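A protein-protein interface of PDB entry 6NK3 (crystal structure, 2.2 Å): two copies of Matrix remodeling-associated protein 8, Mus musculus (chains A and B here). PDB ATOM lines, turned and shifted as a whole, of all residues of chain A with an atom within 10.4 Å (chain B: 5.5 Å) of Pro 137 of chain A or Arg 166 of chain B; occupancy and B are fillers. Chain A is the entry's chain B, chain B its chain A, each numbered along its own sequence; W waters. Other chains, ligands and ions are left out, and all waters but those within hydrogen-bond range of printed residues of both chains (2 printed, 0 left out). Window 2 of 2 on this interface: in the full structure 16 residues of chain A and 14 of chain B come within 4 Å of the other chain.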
ATOM      1  N   ARG A 106     -38.473  23.178  17.796  1.00  0.00           N
ATOM      2  CA  ARG A 106     -38.103  21.830  18.217  1.00  0.00           C
ATOM      3  C   ARG A 106     -39.309  20.900  18.273  1.00  0.00           C
ATOM      4  O   ARG A 106     -39.177  19.701  18.005  1.00  0.00           O
ATOM      5  CB  ARG A 106     -37.404  21.876  19.574  1.00  0.00           C
ATOM      6  CG  ARG A 106     -35.985  22.410  19.509  1.00  0.00           C
ATOM      7  CD  ARG A 106     -34.993  21.364  19.984  1.00  0.00           C
ATOM      8  NE  ARG A 106     -33.619  21.706  19.631  1.00  0.00           N
ATOM      9  CZ  ARG A 106     -32.961  21.189  18.598  1.00  0.00           C
ATOM     10  NH1 ARG A 106     -31.713  21.560  18.354  1.00  0.00           N
ATOM     11  NH2 ARG A 106     -33.550  20.296  17.813  1.00  0.00           N
ATOM     12  N   GLU A 132     -35.552  17.336  10.921  1.00  0.00           N
ATOM     13  CA  GLU A 132     -34.602  17.519  12.008  1.00  0.00           C
ATOM     14  C   GLU A 132     -34.249  18.995  12.114  1.00  0.00           C
ATOM     15  O   GLU A 132     -33.954  19.638  11.102  1.00  0.00           O
ATOM     16  CB  GLU A 132     -33.342  16.679  11.781  1.00  0.00           C
ATOM     17  CG  GLU A 132     -32.265  16.867  12.833  1.00  0.00           C
ATOM     18  CD  GLU A 132     -31.063  15.972  12.596  1.00  0.00           C
ATOM     19  OE1 GLU A 132     -31.185  15.004  11.816  1.00  0.00           O
ATOM     20  OE2 GLU A 132     -29.995  16.239  13.189  1.00  0.00           O
ATOM     21  N   VAL A 133     -34.284  19.525  13.333  1.00  0.00           N
ATOM     22  CA  VAL A 133     -34.003  20.933  13.588  1.00  0.00           C
ATOM     23  C   VAL A 133     -32.557  21.075  14.038  1.00  0.00           C
ATOM     24  O   VAL A 133     -32.109  20.372  14.952  1.00  0.00           O
ATOM     25  CB  VAL A 133     -34.962  21.513  14.640  1.00  0.00           C
ATOM     26  CG1 VAL A 133     -34.537  22.923  15.016  1.00  0.00           C
ATOM     27  CG2 VAL A 133     -36.372  21.512  14.110  1.00  0.00           C
ATOM     28  N   THR A 134     -31.828  21.984  13.398  1.00  0.00           N
ATOM     29  CA  THR A 134     -30.475  22.330  13.797  1.00  0.00           C
ATOM     30  C   THR A 134     -30.428  23.796  14.210  1.00  0.00           C
ATOM     31  O   THR A 134     -31.208  24.620  13.722  1.00  0.00           O
ATOM     32  CB  THR A 134     -29.469  22.067  12.666  1.00  0.00           C
ATOM     33  OG1 THR A 134     -28.145  22.371  13.119  1.00  0.00           O
ATOM     34  CG2 THR A 134     -29.792  22.923  11.454  1.00  0.00           C
ATOM     35  N   GLU A 135     -29.523  24.112  15.132  1.00  0.00           N
ATOM     36  CA  GLU A 135     -29.298  25.489  15.549  1.00  0.00           C
ATOM     37  C   GLU A 135     -28.122  26.131  14.828  1.00  0.00           C
ATOM     38  O   GLU A 135     -27.809  27.296  15.093  1.00  0.00           O
ATOM     39  CB  GLU A 135     -29.091  25.558  17.067  1.00  0.00           C
ATOM     40  CG  GLU A 135     -30.379  25.406  17.865  1.00  0.00           C
ATOM     41  CD  GLU A 135     -30.146  25.386  19.364  1.00  0.00           C
ATOM     42  OE1 GLU A 135     -28.974  25.470  19.786  1.00  0.00           O
ATOM     43  OE2 GLU A 135     -31.135  25.286  20.120  1.00  0.00           O
ATOM     44  N   ASP A 136     -27.470  25.400  13.925  1.00  0.00           N
ATOM     45  CA  ASP A 136     -26.409  25.937  13.081  1.00  0.00           C
ATOM     46  C   ASP A 136     -26.920  25.994  11.648  1.00  0.00           C
ATOM     47  O   ASP A 136     -26.988  24.955  10.973  1.00  0.00           O
ATOM     48  CB  ASP A 136     -25.148  25.069  13.171  1.00  0.00           C
ATOM     49  CG  ASP A 136     -23.978  25.642  12.387  1.00  0.00           C
ATOM     50  OD1 ASP A 136     -24.086  26.774  11.872  1.00  0.00           O
ATOM     51  OD2 ASP A 136     -22.941  24.952  12.285  1.00  0.00           O
ATOM     52  N   PRO A 137     -27.296  27.172  11.140  1.00  0.00           N
ATOM     53  CA  PRO A 137     -27.880  27.242   9.789  1.00  0.00           C
ATOM     54  C   PRO A 137     -26.982  26.690   8.697  1.00  0.00           C
ATOM     55  O   PRO A 137     -27.492  26.295   7.642  1.00  0.00           O
ATOM     56  CB  PRO A 137     -28.135  28.743   9.596  1.00  0.00           C
ATOM     57  CG  PRO A 137     -28.255  29.285  10.979  1.00  0.00           C
ATOM     58  CD  PRO A 137     -27.298  28.481  11.812  1.00  0.00           C
ATOM     59  N   LEU A 138     -25.666  26.649   8.912  1.00  0.00           N
ATOM     60  CA  LEU A 138     -24.770  26.065   7.922  1.00  0.00           C
ATOM     61  C   LEU A 138     -25.012  24.573   7.732  1.00  0.00           C
ATOM     62  O   LEU A 138     -24.672  24.031   6.674  1.00  0.00           O
ATOM     63  CB  LEU A 138     -23.315  26.309   8.325  1.00  0.00           C
ATOM     64  CG  LEU A 138     -22.867  27.771   8.396  1.00  0.00           C
ATOM     65  CD1 LEU A 138     -21.465  27.877   8.979  1.00  0.00           C
ATOM     66  CD2 LEU A 138     -22.932  28.410   7.016  1.00  0.00           C
ATOM     67  N   LEU A 139     -25.591  23.899   8.726  1.00  0.00           N
ATOM     68  CA  LEU A 139     -25.830  22.464   8.655  1.00  0.00           C
ATOM     69  C   LEU A 139     -27.159  22.106   8.002  1.00  0.00           C
ATOM     70  O   LEU A 139     -27.435  20.916   7.810  1.00  0.00           O
ATOM     71  CB  LEU A 139     -25.770  21.849  10.058  1.00  0.00           C
ATOM     72  CG  LEU A 139     -24.449  22.021  10.812  1.00  0.00           C
ATOM     73  CD1 LEU A 139     -24.452  21.204  12.093  1.00  0.00           C
ATOM     74  CD2 LEU A 139     -23.275  21.638   9.927  1.00  0.00           C
ATOM     75  N   SER A 140     -27.982  23.093   7.655  1.00  0.00           N
ATOM     76  CA  SER A 140     -29.258  22.807   7.012  1.00  0.00           C
ATOM     77  C   SER A 140     -29.026  22.150   5.658  1.00  0.00           C
ATOM     78  O   SER A 140     -28.230  22.633   4.848  1.00  0.00           O
ATOM     79  CB  SER A 140     -30.071  24.090   6.844  1.00  0.00           C
ATOM     80  OG  SER A 140     -29.651  24.804   5.690  1.00  0.00           O
ATOM     81  N   ARG A 141     -29.728  21.048   5.413  1.00  0.00           N
ATOM     82  CA  ARG A 141     -29.542  20.277   4.191  1.00  0.00           C
ATOM     83  C   ARG A 141     -30.686  19.280   4.070  1.00  0.00           C
ATOM     84  O   ARG A 141     -31.519  19.144   4.969  1.00  0.00           O
ATOM     85  CB  ARG A 141     -28.196  19.551   4.187  1.00  0.00           C
ATOM     86  CG  ARG A 141     -28.110  18.430   5.207  1.00  0.00           C
ATOM     87  CD  ARG A 141     -26.722  17.822   5.256  1.00  0.00           C
ATOM     88  NE  ARG A 141     -26.674  16.653   6.130  1.00  0.00           N
ATOM     89  CZ  ARG A 141     -26.547  16.714   7.452  1.00  0.00           C
ATOM     90  NH1 ARG A 141     -26.457  17.890   8.055  1.00  0.00           N
ATOM     91  NH2 ARG A 141     -26.514  15.599   8.171  1.00  0.00           N
ATOM     92  N   ALA A 142     -30.707  18.579   2.940  1.00  0.00           N
ATOM     93  CA  ALA A 142     -31.647  17.496   2.695  1.00  0.00           C
ATOM     94  C   ALA A 142     -30.887  16.324   2.097  1.00  0.00           C
ATOM     95  O   ALA A 142     -30.051  16.513   1.208  1.00  0.00           O
ATOM     96  CB  ALA A 142     -32.776  17.935   1.757  1.00  0.00           C
ATOM     97  N   VAL A 152     -32.958  18.623   7.222  1.00  0.00           N
ATOM     98  CA  VAL A 152     -32.348  19.327   8.343  1.00  0.00           C
ATOM     99  C   VAL A 152     -32.598  20.816   8.143  1.00  0.00           C
ATOM    100  O   VAL A 152     -32.200  21.388   7.121  1.00  0.00           O
ATOM    101  CB  VAL A 152     -30.847  19.018   8.450  1.00  0.00           C
ATOM    102  CG1 VAL A 152     -30.263  19.643   9.711  1.00  0.00           C
ATOM    103  CG2 VAL A 152     -30.614  17.513   8.444  1.00  0.00           C
ATOM    104  N   VAL A 153     -33.273  21.441   9.103  1.00  0.00           N
ATOM    105  CA  VAL A 153     -33.745  22.815   8.972  1.00  0.00           C
ATOM    106  C   VAL A 153     -33.248  23.630  10.156  1.00  0.00           C
ATOM    107  O   VAL A 153     -33.306  23.175  11.305  1.00  0.00           O
ATOM    108  CB  VAL A 153     -35.285  22.876   8.879  1.00  0.00           C
ATOM    109  CG1 VAL A 153     -35.784  24.313   8.996  1.00  0.00           C
ATOM    110  CG2 VAL A 153     -35.753  22.258   7.579  1.00  0.00           C
ATOM    111  N   ALA A 154     -32.762  24.835   9.873  1.00  0.00           N
ATOM    112  CA  ALA A 154     -32.341  25.743  10.928  1.00  0.00           C
ATOM    113  C   ALA A 154     -33.536  26.172  11.771  1.00  0.00           C
ATOM    114  O   ALA A 154     -34.624  26.430  11.249  1.00  0.00           O
ATOM    115  CB  ALA A 154     -31.651  26.968  10.333  1.00  0.00           C
ATOM    116  N   HIS A 155     -33.324  26.248  13.086  1.00  0.00           N
ATOM    117  CA  HIS A 155     -34.387  26.627  14.009  1.00  0.00           C
ATOM    118  C   HIS A 155     -34.942  27.998  13.646  1.00  0.00           C
ATOM    119  O   HIS A 155     -34.190  28.950  13.422  1.00  0.00           O
ATOM    120  CB  HIS A 155     -33.856  26.628  15.445  1.00  0.00           C
ATOM    121  CG  HIS A 155     -34.921  26.768  16.489  1.00  0.00           C
ATOM    122  ND1 HIS A 155     -35.602  27.946  16.706  1.00  0.00           N
ATOM    123  CD2 HIS A 155     -35.414  25.879  17.385  1.00  0.00           C
ATOM    124  CE1 HIS A 155     -36.474  27.777  17.684  1.00  0.00           C
ATOM    125  NE2 HIS A 155     -36.379  26.531  18.114  1.00  0.00           N
ATOM    126  N   GLY A 156     -36.268  28.086  13.573  1.00  0.00           N
ATOM    127  CA  GLY A 156     -36.943  29.304  13.196  1.00  0.00           C
ATOM    128  C   GLY A 156     -37.147  29.490  11.707  1.00  0.00           C
ATOM    129  O   GLY A 156     -37.959  30.332  11.307  1.00  0.00           O
ATOM    130  N   ALA A 157     -36.439  28.734  10.876  1.00  0.00           N
ATOM    131  CA  ALA A 157     -36.572  28.891   9.439  1.00  0.00           C
ATOM    132  C   ALA A 157     -37.847  28.216   8.936  1.00  0.00           C
ATOM    133  O   ALA A 157     -38.327  27.251   9.537  1.00  0.00           O
ATOM    134  CB  ALA A 157     -35.368  28.294   8.723  1.00  0.00           C
ATOM    135  N   PRO A 158     -38.421  28.708   7.840  1.00  0.00           N
ATOM    136  CA  PRO A 158     -39.514  27.971   7.200  1.00  0.00           C
ATOM    137  C   PRO A 158     -38.992  26.718   6.516  1.00  0.00           C
ATOM    138  O   PRO A 158     -37.858  26.669   6.036  1.00  0.00           O
ATOM    139  CB  PRO A 158     -40.071  28.972   6.183  1.00  0.00           C
ATOM    140  CG  PRO A 158     -38.904  29.854   5.863  1.00  0.00           C
ATOM    141  CD  PRO A 158     -38.141  29.984   7.157  1.00  0.00           C
ATOM    142  N   ASP B  94     -30.063  34.084  14.484  1.00  0.00           N
ATOM    143  CA  ASP B  94     -29.046  33.130  14.067  1.00  0.00           C
ATOM    144  C   ASP B  94     -28.359  33.504  12.763  1.00  0.00           C
ATOM    145  O   ASP B  94     -27.488  32.755  12.304  1.00  0.00           O
ATOM    146  CB  ASP B  94     -29.656  31.728  13.930  1.00  0.00           C
ATOM    147  CG  ASP B  94     -30.793  31.683  12.926  1.00  0.00           C
ATOM    148  OD1 ASP B  94     -31.443  32.728  12.716  1.00  0.00           O
ATOM    149  OD2 ASP B  94     -31.040  30.602  12.350  1.00  0.00           O
ATOM    150  N   GLY B  95     -28.722  34.627  12.150  1.00  0.00           N
ATOM    151  CA  GLY B  95     -28.081  35.031  10.913  1.00  0.00           C
ATOM    152  C   GLY B  95     -28.522  34.260   9.689  1.00  0.00           C
ATOM    153  O   GLY B  95     -27.776  34.192   8.707  1.00  0.00           O
ATOM    154  N   ASN B  96     -29.718  33.675   9.716  1.00  0.00           N
ATOM    155  CA  ASN B  96     -30.254  32.922   8.581  1.00  0.00           C
ATOM    156  C   ASN B  96     -31.190  33.846   7.809  1.00  0.00           C
ATOM    157  O   ASN B  96     -32.385  33.930   8.090  1.00  0.00           O
ATOM    158  CB  ASN B  96     -30.972  31.659   9.046  1.00  0.00           C
ATOM    159  CG  ASN B  96     -31.512  30.839   7.891  1.00  0.00           C
ATOM    160  OD1 ASN B  96     -31.159  31.071   6.734  1.00  0.00           O
ATOM    161  ND2 ASN B  96     -32.374  29.876   8.198  1.00  0.00           N
ATOM    162  N   ILE B 164     -26.586  33.374   4.583  1.00  0.00           N
ATOM    163  CA  ILE B 164     -26.241  33.107   5.972  1.00  0.00           C
ATOM    164  C   ILE B 164     -25.070  33.994   6.363  1.00  0.00           C
ATOM    165  O   ILE B 164     -24.012  33.952   5.722  1.00  0.00           O
ATOM    166  CB  ILE B 164     -25.897  31.625   6.198  1.00  0.00           C
ATOM    167  CG1 ILE B 164     -27.128  30.745   5.960  1.00  0.00           C
ATOM    168  CG2 ILE B 164     -25.364  31.422   7.596  1.00  0.00           C
ATOM    169  CD1 ILE B 164     -26.872  29.271   6.188  1.00  0.00           C
ATOM    170  N   ASN B 165     -25.258  34.790   7.414  1.00  0.00           N
ATOM    171  CA  ASN B 165     -24.223  35.682   7.936  1.00  0.00           C
ATOM    172  C   ASN B 165     -24.352  35.672   9.456  1.00  0.00           C
ATOM    173  O   ASN B 165     -25.237  36.330  10.012  1.00  0.00           O
ATOM    174  CB  ASN B 165     -24.370  37.089   7.365  1.00  0.00           C
ATOM    175  CG  ASN B 165     -23.128  37.938   7.559  1.00  0.00           C
ATOM    176  OD1 ASN B 165     -22.434  37.831   8.570  1.00  0.00           O
ATOM    177  ND2 ASN B 165     -22.843  38.793   6.583  1.00  0.00           N
ATOM    178  N   ARG B 166     -23.472  34.926  10.123  1.00  0.00           N
ATOM    179  CA  ARG B 166     -23.527  34.753  11.568  1.00  0.00           C
ATOM    180  C   ARG B 166     -22.638  35.736  12.319  1.00  0.00           C
ATOM    181  O   ARG B 166     -22.427  35.563  13.524  1.00  0.00           O
ATOM    182  CB  ARG B 166     -23.147  33.317  11.938  1.00  0.00           C
ATOM    183  CG  ARG B 166     -24.101  32.276  11.375  1.00  0.00           C
ATOM    184  CD  ARG B 166     -23.724  30.866  11.802  1.00  0.00           C
ATOM    185  NE  ARG B 166     -23.635  30.729  13.254  1.00  0.00           N
ATOM    186  CZ  ARG B 166     -24.685  30.696  14.070  1.00  0.00           C
ATOM    187  NH1 ARG B 166     -25.914  30.805  13.584  1.00  0.00           N
ATOM    188  NH2 ARG B 166     -24.504  30.564  15.376  1.00  0.00           N
ATOM    189  N   ALA B 167     -22.117  36.754  11.637  1.00  0.00           N
ATOM    190  CA  ALA B 167     -21.288  37.756  12.296  1.00  0.00           C
ATOM    191  C   ALA B 167     -22.081  38.465  13.386  1.00  0.00           C
ATOM    192  O   ALA B 167     -23.290  38.681  13.259  1.00  0.00           O
ATOM    193  CB  ALA B 167     -20.766  38.765  11.273  1.00  0.00           C
ATOM    194  N   HIS B 168     -21.384  38.833  14.466  1.00  0.00           N
ATOM    195  CA  HIS B 168     -22.062  39.387  15.635  1.00  0.00           C
ATOM    196  C   HIS B 168     -22.732  40.719  15.328  1.00  0.00           C
ATOM    197  O   HIS B 168     -23.702  41.094  15.997  1.00  0.00           O
ATOM    198  CB  HIS B 168     -21.072  39.556  16.786  1.00  0.00           C
ATOM    199  CG  HIS B 168     -20.474  38.272  17.264  1.00  0.00           C
ATOM    200  ND1 HIS B 168     -19.135  37.976  17.123  1.00  0.00           N
ATOM    201  CD2 HIS B 168     -21.031  37.205  17.884  1.00  0.00           C
ATOM    202  CE1 HIS B 168     -18.894  36.783  17.637  1.00  0.00           C
ATOM    203  NE2 HIS B 168     -20.028  36.294  18.105  1.00  0.00           N
ATOM    204  N   THR B 171     -26.223  39.685  14.067  1.00  0.00           N
ATOM    205  CA  THR B 171     -27.024  38.783  14.878  1.00  0.00           C
ATOM    206  C   THR B 171     -27.171  39.310  16.298  1.00  0.00           C
ATOM    207  O   THR B 171     -26.418  40.176  16.750  1.00  0.00           O
ATOM    208  CB  THR B 171     -26.409  37.380  14.900  1.00  0.00           C
ATOM    209  OG1 THR B 171     -25.142  37.423  15.567  1.00  0.00           O
ATOM    210  CG2 THR B 171     -26.214  36.869  13.477  1.00  0.00           C
HETATM  211  O   HOH W   1     -33.663  30.512  11.060  1.00  0.00           O
HETATM  212  O   HOH W   2     -32.728  31.038  15.272  1.00  0.00           O
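Pro 137 of chain A touches three residues of chain B.
Arg 166 of chain B touches one residue of chain A.
Asp 94 of chain B touches just these residues of chain A: Pro 137 and His 155.
No residue of chain A comes within 4 Å of Ala 167 of chain B.
His 168 of chain B touches none of the printed residues of chain A.
Printed residues of chain B within 4 Å of Ala 154 of chain A: Asn 96.
Printed residues of chain B within 4 Å of His 155 of chain A: Asp 94.
Printed residues of chain B within 4 Å of Leu 138 of chain A: Ile 164 (3.9 Å).
Printed residues of chain A within 4 Å of Asn 96 of chain B: Ala 154 and Ala 157.
Pro 158 of chain A touches none of the printed residues of chain B.
The nearest residue of chain B that does not touch Pro 137 of chain A is Asn 96 of chain B (4.1 Å).
The nearest printed residue of chain B that does not touch Ala 157 of chain A is Asp 94 of chain B (5.9 Å).
Of the 19 printed residues of chain A, 5 touch a printed residue of chain B.
Printed residues of chain A that touch a printed residue of chain B: Pro 137, Leu 138, Ala 154, His 155 and Ala 157.
Of the 9 printed residues of chain B, 4 touch a printed residue of chain A.
Hydrophobic or aromatic side chains of chain B that line the printed part of chain A: Ile 164.
Among the printed residues, 7 pairs touch across the chains.
Among the printed residues, no Asp or Glu carboxylate lies within 4 Å of a Lys or Arg side-chain nitrogen of the other chain.
The guanidinium group (NH1) of Arg 166 of chain B lies within hydrogen-bond range of the backbone carbonyl oxygen (O) of Asp 94 of chain B, 2.8 Å away.
The side-chain carboxylate (OD1) of Asp 136 of chain A sits close to the backbone NH (N) of Leu 138 of chain A (3.4 Å).
The backbone carbonyl oxygen (O) of Pro 137 of chain A is in hydrogen-bond range of the side-chain hydroxyl (OG) of Ser 140 of chain A (3.3 Å).
The backbone carbonyl oxygen of Thr 134 of chain A sits at hydrogen-bond distance from the backbone NH of His 155 of chain A (2.7 Å).
Asp 94 of chain B touches Pro 137 of chain A.
Pro 137 of chain A touches Ile 164 of chain B.
Pro 137 of chain A touches Arg 166 of chain B.
Ile 164 of chain B touches Leu 138 of chain A (CG2 to CD2, 3.9 Å).
Asn 96 of chain B touches Ala 154 of chain A.
O of His 155 of chain A touches OD2 of Asp 94 of chain B (3.7 Å).
Asn 96 of chain B touches Ala 157 of chain A (ND2 to CB, 3.4 Å).
No position is printed for both chains.
Of the 7 pairs that touch across the chains among the printed residues, none has its exchanged pair printed and touching as well.
Water W1 lies within hydrogen-bond range of the backbone carbonyl oxygen (O) of His 155 of chain A, the side-chain carboxylate (OD2) of Asp 94 of chain B, the side-chain amide nitrogen (ND2) of Asn 96 of chain B and the backbone NH (N) of Ala 157 of chain A.
Water W2 lies within hydrogen-bond range of the backbone carbonyl oxygen (O) of His 155 of chain A and the side-chain carboxylate (OD1) of Asp 94 of chain B.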
